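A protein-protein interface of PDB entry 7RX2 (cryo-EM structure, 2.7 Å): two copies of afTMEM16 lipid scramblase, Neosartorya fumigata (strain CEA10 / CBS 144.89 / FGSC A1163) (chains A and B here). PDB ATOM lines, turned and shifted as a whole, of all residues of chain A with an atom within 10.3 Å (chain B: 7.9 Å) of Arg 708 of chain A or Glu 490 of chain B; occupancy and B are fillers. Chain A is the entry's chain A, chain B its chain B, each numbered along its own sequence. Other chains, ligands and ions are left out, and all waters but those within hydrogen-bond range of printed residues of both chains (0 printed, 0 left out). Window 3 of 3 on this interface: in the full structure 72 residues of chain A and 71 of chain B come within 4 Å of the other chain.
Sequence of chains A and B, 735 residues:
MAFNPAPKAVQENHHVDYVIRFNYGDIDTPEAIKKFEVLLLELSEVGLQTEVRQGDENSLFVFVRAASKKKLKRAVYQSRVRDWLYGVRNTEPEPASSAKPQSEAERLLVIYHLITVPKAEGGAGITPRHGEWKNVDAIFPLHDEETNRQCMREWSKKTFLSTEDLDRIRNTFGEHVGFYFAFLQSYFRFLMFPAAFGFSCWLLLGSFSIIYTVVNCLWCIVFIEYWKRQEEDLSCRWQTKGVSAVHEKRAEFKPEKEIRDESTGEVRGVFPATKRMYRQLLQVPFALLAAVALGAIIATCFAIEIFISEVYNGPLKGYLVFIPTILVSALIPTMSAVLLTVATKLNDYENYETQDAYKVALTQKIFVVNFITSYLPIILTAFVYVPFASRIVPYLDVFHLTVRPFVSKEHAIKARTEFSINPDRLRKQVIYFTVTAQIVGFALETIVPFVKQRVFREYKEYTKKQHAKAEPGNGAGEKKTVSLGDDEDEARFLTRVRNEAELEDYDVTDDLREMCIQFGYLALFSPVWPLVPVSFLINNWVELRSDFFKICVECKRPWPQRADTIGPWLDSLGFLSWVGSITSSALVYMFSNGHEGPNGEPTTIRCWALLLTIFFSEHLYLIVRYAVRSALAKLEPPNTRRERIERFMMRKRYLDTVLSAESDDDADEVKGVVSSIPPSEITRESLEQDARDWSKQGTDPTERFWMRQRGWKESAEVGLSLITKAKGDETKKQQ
OE1 of Glu 51 of chain B is in salt-bridge range of NH1 of Arg 53 of chain B (2.8 Å). The backbone carbonyl oxygen (O) of Glu 51 of chain B is in hydrogen-bond range of the backbone NH (N) of Phe 63 of chain B (2.8 Å).
No position is printed for both chains. Of the 21 pairs that touch across the chains among the printed residues, none has its exchanged pair printed and touching as well.
Of chain B, only Glu 51 (3.2 Å), Arg 53 (3.5 Å) and Glu 490 (2.3 Å) come within 4 Å of Arg 708 of chain A. Asp 489 of chain B touches none of the printed residues of chain A. No residue of chain A comes within 4 Å of Ala 491 of chain B. No residue of chain A comes within 4 Å of Arg 492 of chain B. Of the printed residues of chain B, Thr 702 of chain A touches His 14. Glu 714 of chain A touches none of the printed residues of chain B. The nearest residue of chain B that does not touch Arg 708 of chain A is Val 52 of chain B (6.4 Å). The nearest printed residue of chain A that does not touch Thr 50 of chain B is Gly 711 of chain A (4.7 Å).
Of the 18 printed residues of chain B, 8 touch a printed residue of chain A. Hydrophobic or aromatic side chains of chain B that line the printed part of chain A: His 14, Val 52 and Phe 63. Printed residues of chain A that touch a printed residue of chain B: Thr 702, Phe 705, Trp 706, Met 707, Arg 708, Gln 709 and Ser 715. Among the printed residues, Asp or Glu carboxylates within 4 Å of a Lys or Arg side-chain nitrogen of the other chain: Arg 708 of chain A with Glu 490 of chain B (2.3 Å).
OE2 of Glu 51 of chain B is in hydrogen-bond range of N of Gln 709 of chain A (3.1 Å). NH1 of Arg 53 of chain B lies close to NE2 of Gln 709 of chain A. The guanidinium group (NH2) of Arg 53 of chain B is in hydrogen-bond range of the backbone carbonyl oxygen (O) of Phe 705 of chain A (3.4 Å). The side-chain carboxylate (OE2) of Glu 51 of chain B sits close to the backbone carbonyl oxygen (O) of Trp 706 of chain A (2.7 Å). NE1 of Trp 706 of chain A is in hydrogen-bond range of O of His 14 of chain B (2.7 Å). O of Phe 705 of chain A sits close to OE2 of Glu 51 of chain B (3.3 Å). The backbone NH (N) of Arg 708 of chain A is in hydrogen-bond range of the side-chain carboxylate (OE2) of Glu 51 of chain B (3.2 Å). The side-chain amide nitrogen (NE2) of Gln 709 of chain A is in hydrogen-bond range of the backbone carbonyl oxygen (O) of Val 52 of chain B (2.9 Å).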
ATOM      1  N   PRO A 701       3.416  14.899  -0.834  1.00  0.00           N
ATOM      2  CA  PRO A 701       2.000  14.755  -0.492  1.00  0.00           C
ATOM      3  C   PRO A 701       1.303  16.102  -0.388  1.00  0.00           C
ATOM      4  O   PRO A 701       1.212  16.819  -1.381  1.00  0.00           O
ATOM      5  CB  PRO A 701       2.044  14.051   0.864  1.00  0.00           C
ATOM      6  CG  PRO A 701       3.303  14.519   1.472  1.00  0.00           C
ATOM      7  CD  PRO A 701       4.284  14.667   0.331  1.00  0.00           C
ATOM      8  N   THR A 702       0.823  16.444   0.809  1.00  0.00           N
ATOM      9  CA  THR A 702       0.157  17.728   0.983  1.00  0.00           C
ATOM     10  C   THR A 702       1.141  18.883   0.887  1.00  0.00           C
ATOM     11  O   THR A 702       0.810  19.925   0.314  1.00  0.00           O
ATOM     12  CB  THR A 702      -0.570  17.780   2.323  1.00  0.00           C
ATOM     13  OG1 THR A 702       0.331  18.227   3.344  1.00  0.00           O
ATOM     14  CG2 THR A 702      -1.092  16.405   2.688  1.00  0.00           C
ATOM     15  N   GLU A 703       2.353  18.716   1.424  1.00  0.00           N
ATOM     16  CA  GLU A 703       3.324  19.804   1.443  1.00  0.00           C
ATOM     17  C   GLU A 703       3.714  20.267   0.046  1.00  0.00           C
ATOM     18  O   GLU A 703       4.225  21.380  -0.100  1.00  0.00           O
ATOM     19  CB  GLU A 703       4.569  19.386   2.220  1.00  0.00           C
ATOM     20  N   ARG A 704       3.488  19.443  -0.977  1.00  0.00           N
ATOM     21  CA  ARG A 704       3.629  19.894  -2.353  1.00  0.00           C
ATOM     22  C   ARG A 704       2.661  21.019  -2.683  1.00  0.00           C
ATOM     23  O   ARG A 704       2.937  21.811  -3.587  1.00  0.00           O
ATOM     24  CB  ARG A 704       3.405  18.722  -3.300  1.00  0.00           C
ATOM     25  CG  ARG A 704       4.296  18.706  -4.520  1.00  0.00           C
ATOM     26  CD  ARG A 704       4.422  17.290  -5.057  1.00  0.00           C
ATOM     27  NE  ARG A 704       5.045  16.396  -4.085  1.00  0.00           N
ATOM     28  CZ  ARG A 704       4.887  15.078  -4.068  1.00  0.00           C
ATOM     29  NH1 ARG A 704       4.108  14.489  -4.965  1.00  0.00           N
ATOM     30  NH2 ARG A 704       5.500  14.348  -3.146  1.00  0.00           N
ATOM     31  N   PHE A 705       1.534  21.095  -1.978  1.00  0.00           N
ATOM     32  CA  PHE A 705       0.599  22.199  -2.159  1.00  0.00           C
ATOM     33  C   PHE A 705       1.237  23.532  -1.802  1.00  0.00           C
ATOM     34  O   PHE A 705       0.951  24.546  -2.446  1.00  0.00           O
ATOM     35  CB  PHE A 705      -0.645  21.946  -1.303  1.00  0.00           C
ATOM     36  CG  PHE A 705      -1.675  23.028  -1.371  1.00  0.00           C
ATOM     37  CD1 PHE A 705      -2.634  23.019  -2.356  1.00  0.00           C
ATOM     38  CD2 PHE A 705      -1.705  24.039  -0.431  1.00  0.00           C
ATOM     39  CE1 PHE A 705      -3.584  24.004  -2.415  1.00  0.00           C
ATOM     40  CE2 PHE A 705      -2.654  25.023  -0.492  1.00  0.00           C
ATOM     41  CZ  PHE A 705      -3.595  25.004  -1.485  1.00  0.00           C
ATOM     42  N   TRP A 706       2.105  23.551  -0.799  1.00  0.00           N
ATOM     43  CA  TRP A 706       2.641  24.785  -0.249  1.00  0.00           C
ATOM     44  C   TRP A 706       4.036  25.114  -0.752  1.00  0.00           C
ATOM     45  O   TRP A 706       4.505  26.233  -0.534  1.00  0.00           O
ATOM     46  CB  TRP A 706       2.656  24.718   1.274  1.00  0.00           C
ATOM     47  CG  TRP A 706       1.306  24.644   1.876  1.00  0.00           C
ATOM     48  CD1 TRP A 706       0.613  23.522   2.182  1.00  0.00           C
ATOM     49  CD2 TRP A 706       0.480  25.744   2.251  1.00  0.00           C
ATOM     50  NE1 TRP A 706      -0.596  23.848   2.728  1.00  0.00           N
ATOM     51  CE2 TRP A 706      -0.703  25.212   2.776  1.00  0.00           C
ATOM     52  CE3 TRP A 706       0.626  27.127   2.190  1.00  0.00           C
ATOM     53  CZ2 TRP A 706      -1.729  26.010   3.238  1.00  0.00           C
ATOM     54  CZ3 TRP A 706      -0.390  27.914   2.646  1.00  0.00           C
ATOM     55  CH2 TRP A 706      -1.555  27.357   3.165  1.00  0.00           C
ATOM     56  N   MET A 707       4.709  24.175  -1.414  1.00  0.00           N
ATOM     57  CA  MET A 707       5.988  24.455  -2.051  1.00  0.00           C
ATOM     58  C   MET A 707       5.830  25.206  -3.363  1.00  0.00           C
ATOM     59  O   MET A 707       6.831  25.463  -4.035  1.00  0.00           O
ATOM     60  CB  MET A 707       6.751  23.153  -2.311  1.00  0.00           C
ATOM     61  CG  MET A 707       7.133  22.358  -1.078  1.00  0.00           C
ATOM     62  SD  MET A 707       8.306  23.169   0.021  1.00  0.00           S
ATOM     63  CE  MET A 707       8.325  22.006   1.385  1.00  0.00           C
ATOM     64  N   ARG A 708       4.602  25.553  -3.739  1.00  0.00           N
ATOM     65  CA  ARG A 708       4.346  26.140  -5.047  1.00  0.00           C
ATOM     66  C   ARG A 708       4.913  27.549  -5.148  1.00  0.00           C
ATOM     67  O   ARG A 708       5.796  27.816  -5.969  1.00  0.00           O
ATOM     68  CB  ARG A 708       2.843  26.139  -5.316  1.00  0.00           C
ATOM     69  CG  ARG A 708       2.459  26.381  -6.746  1.00  0.00           C
ATOM     70  CD  ARG A 708       2.545  25.107  -7.539  1.00  0.00           C
ATOM     71  NE  ARG A 708       1.536  24.139  -7.123  1.00  0.00           N
ATOM     72  CZ  ARG A 708       1.601  22.844  -7.402  1.00  0.00           C
ATOM     73  NH1 ARG A 708       2.630  22.370  -8.092  1.00  0.00           N
ATOM     74  NH2 ARG A 708       0.644  22.024  -6.990  1.00  0.00           N
ATOM     75  N   GLN A 709       4.417  28.466  -4.323  1.00  0.00           N
ATOM     76  CA  GLN A 709       4.781  29.879  -4.388  1.00  0.00           C
ATOM     77  C   GLN A 709       5.477  30.253  -3.089  1.00  0.00           C
ATOM     78  O   GLN A 709       4.826  30.390  -2.050  1.00  0.00           O
ATOM     79  CB  GLN A 709       3.544  30.742  -4.622  1.00  0.00           C
ATOM     80  CG  GLN A 709       2.543  30.107  -5.558  1.00  0.00           C
ATOM     81  CD  GLN A 709       1.156  30.679  -5.411  1.00  0.00           C
ATOM     82  OE1 GLN A 709       0.981  31.771  -4.886  1.00  0.00           O
ATOM     83  NE2 GLN A 709       0.159  29.939  -5.870  1.00  0.00           N
ATOM     84  N   ARG A 710       6.795  30.437  -3.149  1.00  0.00           N
ATOM     85  CA  ARG A 710       7.595  30.498  -1.929  1.00  0.00           C
ATOM     86  C   ARG A 710       7.301  31.753  -1.123  1.00  0.00           C
ATOM     87  O   ARG A 710       6.780  31.678  -0.005  1.00  0.00           O
ATOM     88  CB  ARG A 710       9.084  30.425  -2.274  1.00  0.00           C
ATOM     89  N   GLY A 711       7.610  32.918  -1.676  1.00  0.00           N
ATOM     90  CA  GLY A 711       7.437  34.167  -0.969  1.00  0.00           C
ATOM     91  C   GLY A 711       6.021  34.682  -1.074  1.00  0.00           C
ATOM     92  O   GLY A 711       5.095  33.979  -1.480  1.00  0.00           O
ATOM     93  N   TRP A 712       5.856  35.937  -0.683  1.00  0.00           N
ATOM     94  CA  TRP A 712       4.608  36.627  -0.945  1.00  0.00           C
ATOM     95  C   TRP A 712       4.611  37.326  -2.292  1.00  0.00           C
ATOM     96  O   TRP A 712       3.544  37.730  -2.760  1.00  0.00           O
ATOM     97  CB  TRP A 712       4.297  37.635   0.173  1.00  0.00           C
ATOM     98  CG  TRP A 712       5.135  38.874   0.196  1.00  0.00           C
ATOM     99  CD1 TRP A 712       6.238  39.100   0.961  1.00  0.00           C
ATOM    100  CD2 TRP A 712       4.917  40.073  -0.555  1.00  0.00           C
ATOM    101  NE1 TRP A 712       6.729  40.361   0.724  1.00  0.00           N
ATOM    102  CE2 TRP A 712       5.935  40.975  -0.208  1.00  0.00           C
ATOM    103  CE3 TRP A 712       3.966  40.463  -1.500  1.00  0.00           C
ATOM    104  CZ2 TRP A 712       6.028  42.243  -0.769  1.00  0.00           C
ATOM    105  CZ3 TRP A 712       4.058  41.718  -2.052  1.00  0.00           C
ATOM    106  CH2 TRP A 712       5.079  42.597  -1.684  1.00  0.00           C
ATOM    107  N   LYS A 713       5.775  37.468  -2.928  1.00  0.00           N
ATOM    108  CA  LYS A 713       5.807  38.054  -4.262  1.00  0.00           C
ATOM    109  C   LYS A 713       5.321  37.067  -5.306  1.00  0.00           C
ATOM    110  O   LYS A 713       4.564  37.445  -6.204  1.00  0.00           O
ATOM    111  CB  LYS A 713       7.210  38.538  -4.615  1.00  0.00           C
ATOM    112  CG  LYS A 713       7.677  39.724  -3.810  1.00  0.00           C
ATOM    113  CD  LYS A 713       6.702  40.871  -3.980  1.00  0.00           C
ATOM    114  CE  LYS A 713       6.668  41.379  -5.408  1.00  0.00           C
ATOM    115  NZ  LYS A 713       7.010  42.826  -5.480  1.00  0.00           N
ATOM    116  N   GLU A 714       5.718  35.797  -5.187  1.00  0.00           N
ATOM    117  CA  GLU A 714       5.245  34.787  -6.125  1.00  0.00           C
ATOM    118  C   GLU A 714       3.737  34.624  -6.058  1.00  0.00           C
ATOM    119  O   GLU A 714       3.085  34.533  -7.102  1.00  0.00           O
ATOM    120  CB  GLU A 714       5.924  33.451  -5.854  1.00  0.00           C
ATOM    121  CG  GLU A 714       7.338  33.368  -6.367  1.00  0.00           C
ATOM    122  CD  GLU A 714       8.011  32.075  -5.977  1.00  0.00           C
ATOM    123  OE1 GLU A 714       8.658  31.461  -6.848  1.00  0.00           O
ATOM    124  OE2 GLU A 714       7.895  31.675  -4.799  1.00  0.00           O
ATOM    125  N   SER A 715       3.165  34.589  -4.850  1.00  0.00           N
ATOM    126  CA  SER A 715       1.714  34.659  -4.720  1.00  0.00           C
ATOM    127  C   SER A 715       1.167  35.914  -5.380  1.00  0.00           C
ATOM    128  O   SER A 715       0.118  35.867  -6.027  1.00  0.00           O
ATOM    129  CB  SER A 715       1.307  34.626  -3.245  1.00  0.00           C
ATOM    130  OG  SER A 715       1.887  33.531  -2.557  1.00  0.00           O
ATOM    131  N   ALA A 716       1.878  37.030  -5.249  1.00  0.00           N
ATOM    132  CA  ALA A 716       1.445  38.284  -5.851  1.00  0.00           C
ATOM    133  C   ALA A 716       1.402  38.209  -7.373  1.00  0.00           C
ATOM    134  O   ALA A 716       0.502  38.786  -7.990  1.00  0.00           O
ATOM    135  CB  ALA A 716       2.365  39.415  -5.402  1.00  0.00           C
ATOM    136  N   VAL A 718       1.261  35.250  -9.194  1.00  0.00           N
ATOM    137  CA  VAL A 718       0.272  34.243  -9.537  1.00  0.00           C
ATOM    138  C   VAL A 718      -1.124  34.833  -9.469  1.00  0.00           C
ATOM    139  O   VAL A 718      -2.015  34.413 -10.212  1.00  0.00           O
ATOM    140  CB  VAL A 718       0.416  33.028  -8.610  1.00  0.00           C
ATOM    141  CG1 VAL A 718      -0.629  31.993  -8.935  1.00  0.00           C
ATOM    142  CG2 VAL A 718       1.815  32.438  -8.724  1.00  0.00           C
ATOM    143  N   LEU A 722      -3.872  35.492 -12.880  1.00  0.00           N
ATOM    144  CA  LEU A 722      -5.262  35.068 -12.842  1.00  0.00           C
ATOM    145  C   LEU A 722      -6.235  36.228 -12.860  1.00  0.00           C
ATOM    146  O   LEU A 722      -7.302  36.113 -13.467  1.00  0.00           O
ATOM    147  CB  LEU A 722      -5.526  34.228 -11.592  1.00  0.00           C
ATOM    148  CG  LEU A 722      -4.937  32.827 -11.571  1.00  0.00           C
ATOM    149  CD1 LEU A 722      -5.109  32.223 -10.196  1.00  0.00           C
ATOM    150  CD2 LEU A 722      -5.607  31.970 -12.617  1.00  0.00           C
ATOM    151  N   HIS B  14      -4.691  19.495   4.053  1.00  0.00           N
ATOM    152  CA  HIS B  14      -3.482  20.101   3.504  1.00  0.00           C
ATOM    153  C   HIS B  14      -2.887  21.140   4.445  1.00  0.00           C
ATOM    154  O   HIS B  14      -2.166  22.040   4.016  1.00  0.00           O
ATOM    155  CB  HIS B  14      -3.750  20.711   2.130  1.00  0.00           C
ATOM    156  CG  HIS B  14      -4.017  19.698   1.063  1.00  0.00           C
ATOM    157  ND1 HIS B  14      -3.344  19.688  -0.138  1.00  0.00           N
ATOM    158  CD2 HIS B  14      -4.881  18.657   1.016  1.00  0.00           C
ATOM    159  CE1 HIS B  14      -3.783  18.688  -0.879  1.00  0.00           C
ATOM    160  NE2 HIS B  14      -4.716  18.047  -0.201  1.00  0.00           N
ATOM    161  N   GLN B  49       1.823  31.877   6.033  1.00  0.00           N
ATOM    162  CA  GLN B  49       2.245  31.412   4.724  1.00  0.00           C
ATOM    163  C   GLN B  49       1.032  31.289   3.819  1.00  0.00           C
ATOM    164  O   GLN B  49      -0.027  30.833   4.251  1.00  0.00           O
ATOM    165  CB  GLN B  49       2.956  30.069   4.839  1.00  0.00           C
ATOM    166  CG  GLN B  49       3.481  29.539   3.541  1.00  0.00           C
ATOM    167  CD  GLN B  49       4.133  28.200   3.703  1.00  0.00           C
ATOM    168  OE1 GLN B  49       4.087  27.602   4.771  1.00  0.00           O
ATOM    169  NE2 GLN B  49       4.755  27.715   2.642  1.00  0.00           N
ATOM    170  N   THR B  50       1.184  31.693   2.562  1.00  0.00           N
ATOM    171  CA  THR B  50       0.051  31.825   1.662  1.00  0.00           C
ATOM    172  C   THR B  50       0.267  31.051   0.370  1.00  0.00           C
ATOM    173  O   THR B  50       1.397  30.857  -0.080  1.00  0.00           O
ATOM    174  CB  THR B  50      -0.215  33.285   1.328  1.00  0.00           C
ATOM    175  OG1 THR B  50       0.980  33.877   0.815  1.00  0.00           O
ATOM    176  CG2 THR B  50      -0.647  34.036   2.561  1.00  0.00           C
ATOM    177  N   GLU B  51      -0.842  30.618  -0.217  1.00  0.00           N
ATOM    178  CA  GLU B  51      -0.871  29.986  -1.525  1.00  0.00           C
ATOM    179  C   GLU B  51      -2.135  30.443  -2.229  1.00  0.00           C
ATOM    180  O   GLU B  51      -3.232  30.261  -1.703  1.00  0.00           O
ATOM    181  CB  GLU B  51      -0.849  28.463  -1.411  1.00  0.00           C
ATOM    182  CG  GLU B  51       0.506  27.887  -1.066  1.00  0.00           C
ATOM    183  CD  GLU B  51       1.396  27.703  -2.284  1.00  0.00           C
ATOM    184  OE1 GLU B  51       0.907  27.887  -3.414  1.00  0.00           O
ATOM    185  OE2 GLU B  51       2.585  27.376  -2.106  1.00  0.00           O
ATOM    186  N   VAL B  52      -1.984  31.032  -3.409  1.00  0.00           N
ATOM    187  CA  VAL B  52      -3.091  31.626  -4.144  1.00  0.00           C
ATOM    188  C   VAL B  52      -3.559  30.642  -5.203  1.00  0.00           C
ATOM    189  O   VAL B  52      -2.739  29.996  -5.862  1.00  0.00           O
ATOM    190  CB  VAL B  52      -2.686  32.963  -4.781  1.00  0.00           C
ATOM    191  CG1 VAL B  52      -3.817  33.501  -5.615  1.00  0.00           C
ATOM    192  CG2 VAL B  52      -2.297  33.947  -3.714  1.00  0.00           C
ATOM    193  N   ARG B  53      -4.873  30.525  -5.358  1.00  0.00           N
ATOM    194  CA  ARG B  53      -5.496  29.689  -6.371  1.00  0.00           C
ATOM    195  C   ARG B  53      -6.722  30.405  -6.904  1.00  0.00           C
ATOM    196  O   ARG B  53      -7.125  31.450  -6.395  1.00  0.00           O
ATOM    197  CB  ARG B  53      -5.889  28.320  -5.819  1.00  0.00           C
ATOM    198  CG  ARG B  53      -4.741  27.542  -5.248  1.00  0.00           C
ATOM    199  CD  ARG B  53      -3.716  27.216  -6.302  1.00  0.00           C
ATOM    200  NE  ARG B  53      -2.971  26.017  -5.943  1.00  0.00           N
ATOM    201  CZ  ARG B  53      -1.791  26.026  -5.340  1.00  0.00           C
ATOM    202  NH1 ARG B  53      -1.206  27.170  -5.033  1.00  0.00           N
ATOM    203  NH2 ARG B  53      -1.193  24.886  -5.049  1.00  0.00           N
ATOM    204  N   PHE B  63      -4.986  30.776   0.466  1.00  0.00           N
ATOM    205  CA  PHE B  63      -4.886  29.771   1.509  1.00  0.00           C
ATOM    206  C   PHE B  63      -3.800  30.170   2.493  1.00  0.00           C
ATOM    207  O   PHE B  63      -2.684  30.503   2.097  1.00  0.00           O
ATOM    208  CB  PHE B  63      -4.588  28.399   0.916  1.00  0.00           C
ATOM    209  CG  PHE B  63      -5.703  27.854   0.093  1.00  0.00           C
ATOM    210  CD1 PHE B  63      -5.838  28.207  -1.230  1.00  0.00           C
ATOM    211  CD2 PHE B  63      -6.633  27.004   0.647  1.00  0.00           C
ATOM    212  CE1 PHE B  63      -6.864  27.715  -1.980  1.00  0.00           C
ATOM    213  CE2 PHE B  63      -7.660  26.512  -0.105  1.00  0.00           C
ATOM    214  CZ  PHE B  63      -7.775  26.869  -1.420  1.00  0.00           C
ATOM    215  N   GLU B 488      -3.520  18.095 -10.552  1.00  0.00           N
ATOM    216  CA  GLU B 488      -3.910  16.690 -10.602  1.00  0.00           C
ATOM    217  C   GLU B 488      -4.215  16.158  -9.207  1.00  0.00           C
ATOM    218  O   GLU B 488      -5.308  15.654  -8.951  1.00  0.00           O
ATOM    219  CB  GLU B 488      -2.814  15.850 -11.257  1.00  0.00           C
ATOM    220  N   ASP B 489      -3.240  16.268  -8.305  1.00  0.00           N
ATOM    221  CA  ASP B 489      -3.469  15.874  -6.920  1.00  0.00           C
ATOM    222  C   ASP B 489      -4.320  16.901  -6.179  1.00  0.00           C
ATOM    223  O   ASP B 489      -5.206  16.533  -5.400  1.00  0.00           O
ATOM    224  CB  ASP B 489      -2.133  15.676  -6.202  1.00  0.00           C
ATOM    225  N   GLU B 490      -4.066  18.185  -6.403  1.00  0.00           N
ATOM    226  CA  GLU B 490      -4.806  19.243  -5.736  1.00  0.00           C
ATOM    227  C   GLU B 490      -6.030  19.688  -6.524  1.00  0.00           C
ATOM    228  O   GLU B 490      -6.454  20.838  -6.389  1.00  0.00           O
ATOM    229  CB  GLU B 490      -3.886  20.432  -5.455  1.00  0.00           C
ATOM    230  CG  GLU B 490      -3.531  21.259  -6.671  1.00  0.00           C
ATOM    231  CD  GLU B 490      -2.441  22.269  -6.382  1.00  0.00           C
ATOM    232  OE1 GLU B 490      -1.355  21.863  -5.923  1.00  0.00           O
ATOM    233  OE2 GLU B 490      -2.676  23.473  -6.598  1.00  0.00           O
ATOM    234  N   ALA B 491      -6.603  18.807  -7.342  1.00  0.00           N
ATOM    235  CA  ALA B 491      -7.807  19.151  -8.087  1.00  0.00           C
ATOM    236  C   ALA B 491      -9.067  18.651  -7.401  1.00  0.00           C
ATOM    237  O   ALA B 491     -10.135  19.243  -7.572  1.00  0.00           O
ATOM    238  CB  ALA B 491      -7.729  18.589  -9.501  1.00  0.00           C
ATOM    239  N   ARG B 492      -8.973  17.555  -6.652  1.00  0.00           N
ATOM    240  CA  ARG B 492     -10.110  17.109  -5.863  1.00  0.00           C
ATOM    241  C   ARG B 492     -10.268  17.944  -4.605  1.00  0.00           C
ATOM    242  O   ARG B 492     -11.395  18.250  -4.205  1.00  0.00           O
ATOM    243  CB  ARG B 492      -9.958  15.634  -5.499  1.00  0.00           C
ATOM    244  N   PHE B 493      -9.150  18.328  -3.987  1.00  0.00           N
ATOM    245  CA  PHE B 493      -9.205  19.197  -2.823  1.00  0.00           C
ATOM    246  C   PHE B 493      -9.715  20.580  -3.194  1.00  0.00           C
ATOM    247  O   PHE B 493     -10.603  21.118  -2.526  1.00  0.00           O
ATOM    248  CB  PHE B 493      -7.825  19.292  -2.182  1.00  0.00           C
ATOM    249  CG  PHE B 493      -7.701  20.386  -1.170  1.00  0.00           C
ATOM    250  CD1 PHE B 493      -8.305  20.274   0.062  1.00  0.00           C
ATOM    251  CD2 PHE B 493      -6.977  21.525  -1.451  1.00  0.00           C
ATOM    252  CE1 PHE B 493      -8.192  21.277   0.988  1.00  0.00           C
ATOM    253  CE2 PHE B 493      -6.860  22.521  -0.526  1.00  0.00           C
ATOM    254  CZ  PHE B 493      -7.471  22.397   0.695  1.00  0.00           C
ATOM    255  N   LEU B 494      -9.172  21.173  -4.252  1.00  0.00           N
ATOM    256  CA  LEU B 494      -9.632  22.492  -4.659  1.00  0.00           C
ATOM    257  C   LEU B 494     -11.073  22.474  -5.128  1.00  0.00           C
ATOM    258  O   LEU B 494     -11.750  23.500  -5.049  1.00  0.00           O
ATOM    259  CB  LEU B 494      -8.742  23.047  -5.761  1.00  0.00           C
ATOM    260  CG  LEU B 494      -7.382  23.545  -5.304  1.00  0.00           C
ATOM    261  CD1 LEU B 494      -6.538  23.877  -6.505  1.00  0.00           C
ATOM    262  CD2 LEU B 494      -7.558  24.758  -4.417  1.00  0.00           C
ATOM    263  N   THR B 495     -11.555  21.334  -5.614  1.00  0.00           N
ATOM    264  CA  THR B 495     -12.946  21.252  -6.038  1.00  0.00           C
ATOM    265  C   THR B 495     -13.890  21.349  -4.850  1.00  0.00           C
ATOM    266  O   THR B 495     -14.956  21.964  -4.949  1.00  0.00           O
ATOM    267  CB  THR B 495     -13.184  19.954  -6.803  1.00  0.00           C
ATOM    268  OG1 THR B 495     -12.542  20.034  -8.080  1.00  0.00           O
ATOM    269  CG2 THR B 495     -14.664  19.727  -7.001  1.00  0.00           C
ATOM    270  N   ARG B 496     -13.525  20.744  -3.725  1.00  0.00           N
ATOM    271  CA  ARG B 496     -14.391  20.798  -2.561  1.00  0.00           C
ATOM    272  C   ARG B 496     -14.210  22.069  -1.753  1.00  0.00           C
ATOM    273  O   ARG B 496     -15.099  22.414  -0.975  1.00  0.00           O
ATOM    274  CB  ARG B 496     -14.165  19.586  -1.664  1.00  0.00           C
ATOM    275  CG  ARG B 496     -12.806  19.504  -1.050  1.00  0.00           C
ATOM    276  CD  ARG B 496     -12.841  18.600   0.156  1.00  0.00           C
ATOM    277  NE  ARG B 496     -13.233  19.310   1.367  1.00  0.00           N
ATOM    278  CZ  ARG B 496     -12.399  19.592   2.361  1.00  0.00           C
ATOM    279  NH1 ARG B 496     -12.831  20.242   3.430  1.00  0.00           N
ATOM    280  NH2 ARG B 496     -11.130  19.223   2.282  1.00  0.00           N
ATOM    281  N   VAL B 497     -13.086  22.769  -1.905  1.00  0.00           N
ATOM    282  CA  VAL B 497     -12.968  24.082  -1.284  1.00  0.00           C
ATOM    283  C   VAL B 497     -13.861  25.080  -1.999  1.00  0.00           C
ATOM    284  O   VAL B 497     -14.358  26.033  -1.391  1.00  0.00           O
ATOM    285  CB  VAL B 497     -11.507  24.557  -1.260  1.00  0.00           C
ATOM    286  CG1 VAL B 497     -11.428  25.923  -0.625  1.00  0.00           C
ATOM    287  CG2 VAL B 497     -10.656  23.594  -0.495  1.00  0.00           C
ATOM    288  N   ARG B 498     -14.079  24.885  -3.298  1.00  0.00           N
ATOM    289  CA  ARG B 498     -15.015  25.741  -4.012  1.00  0.00           C
ATOM    290  C   ARG B 498     -16.456  25.396  -3.668  1.00  0.00           C
ATOM    291  O   ARG B 498     -17.340  26.247  -3.788  1.00  0.00           O
ATOM    292  CB  ARG B 498     -14.781  25.639  -5.517  1.00  0.00           C
ATOM    293  CG  ARG B 498     -13.392  26.064  -5.941  1.00  0.00           C
ATOM    294  CD  ARG B 498     -13.239  26.115  -7.447  1.00  0.00           C
ATOM    295  NE  ARG B 498     -11.921  26.606  -7.828  1.00  0.00           N
ATOM    296  CZ  ARG B 498     -10.884  25.827  -8.106  1.00  0.00           C
ATOM    297  NH1 ARG B 498      -9.723  26.362  -8.430  1.00  0.00           N
ATOM    298  NH2 ARG B 498     -11.008  24.513  -8.061  1.00  0.00           N
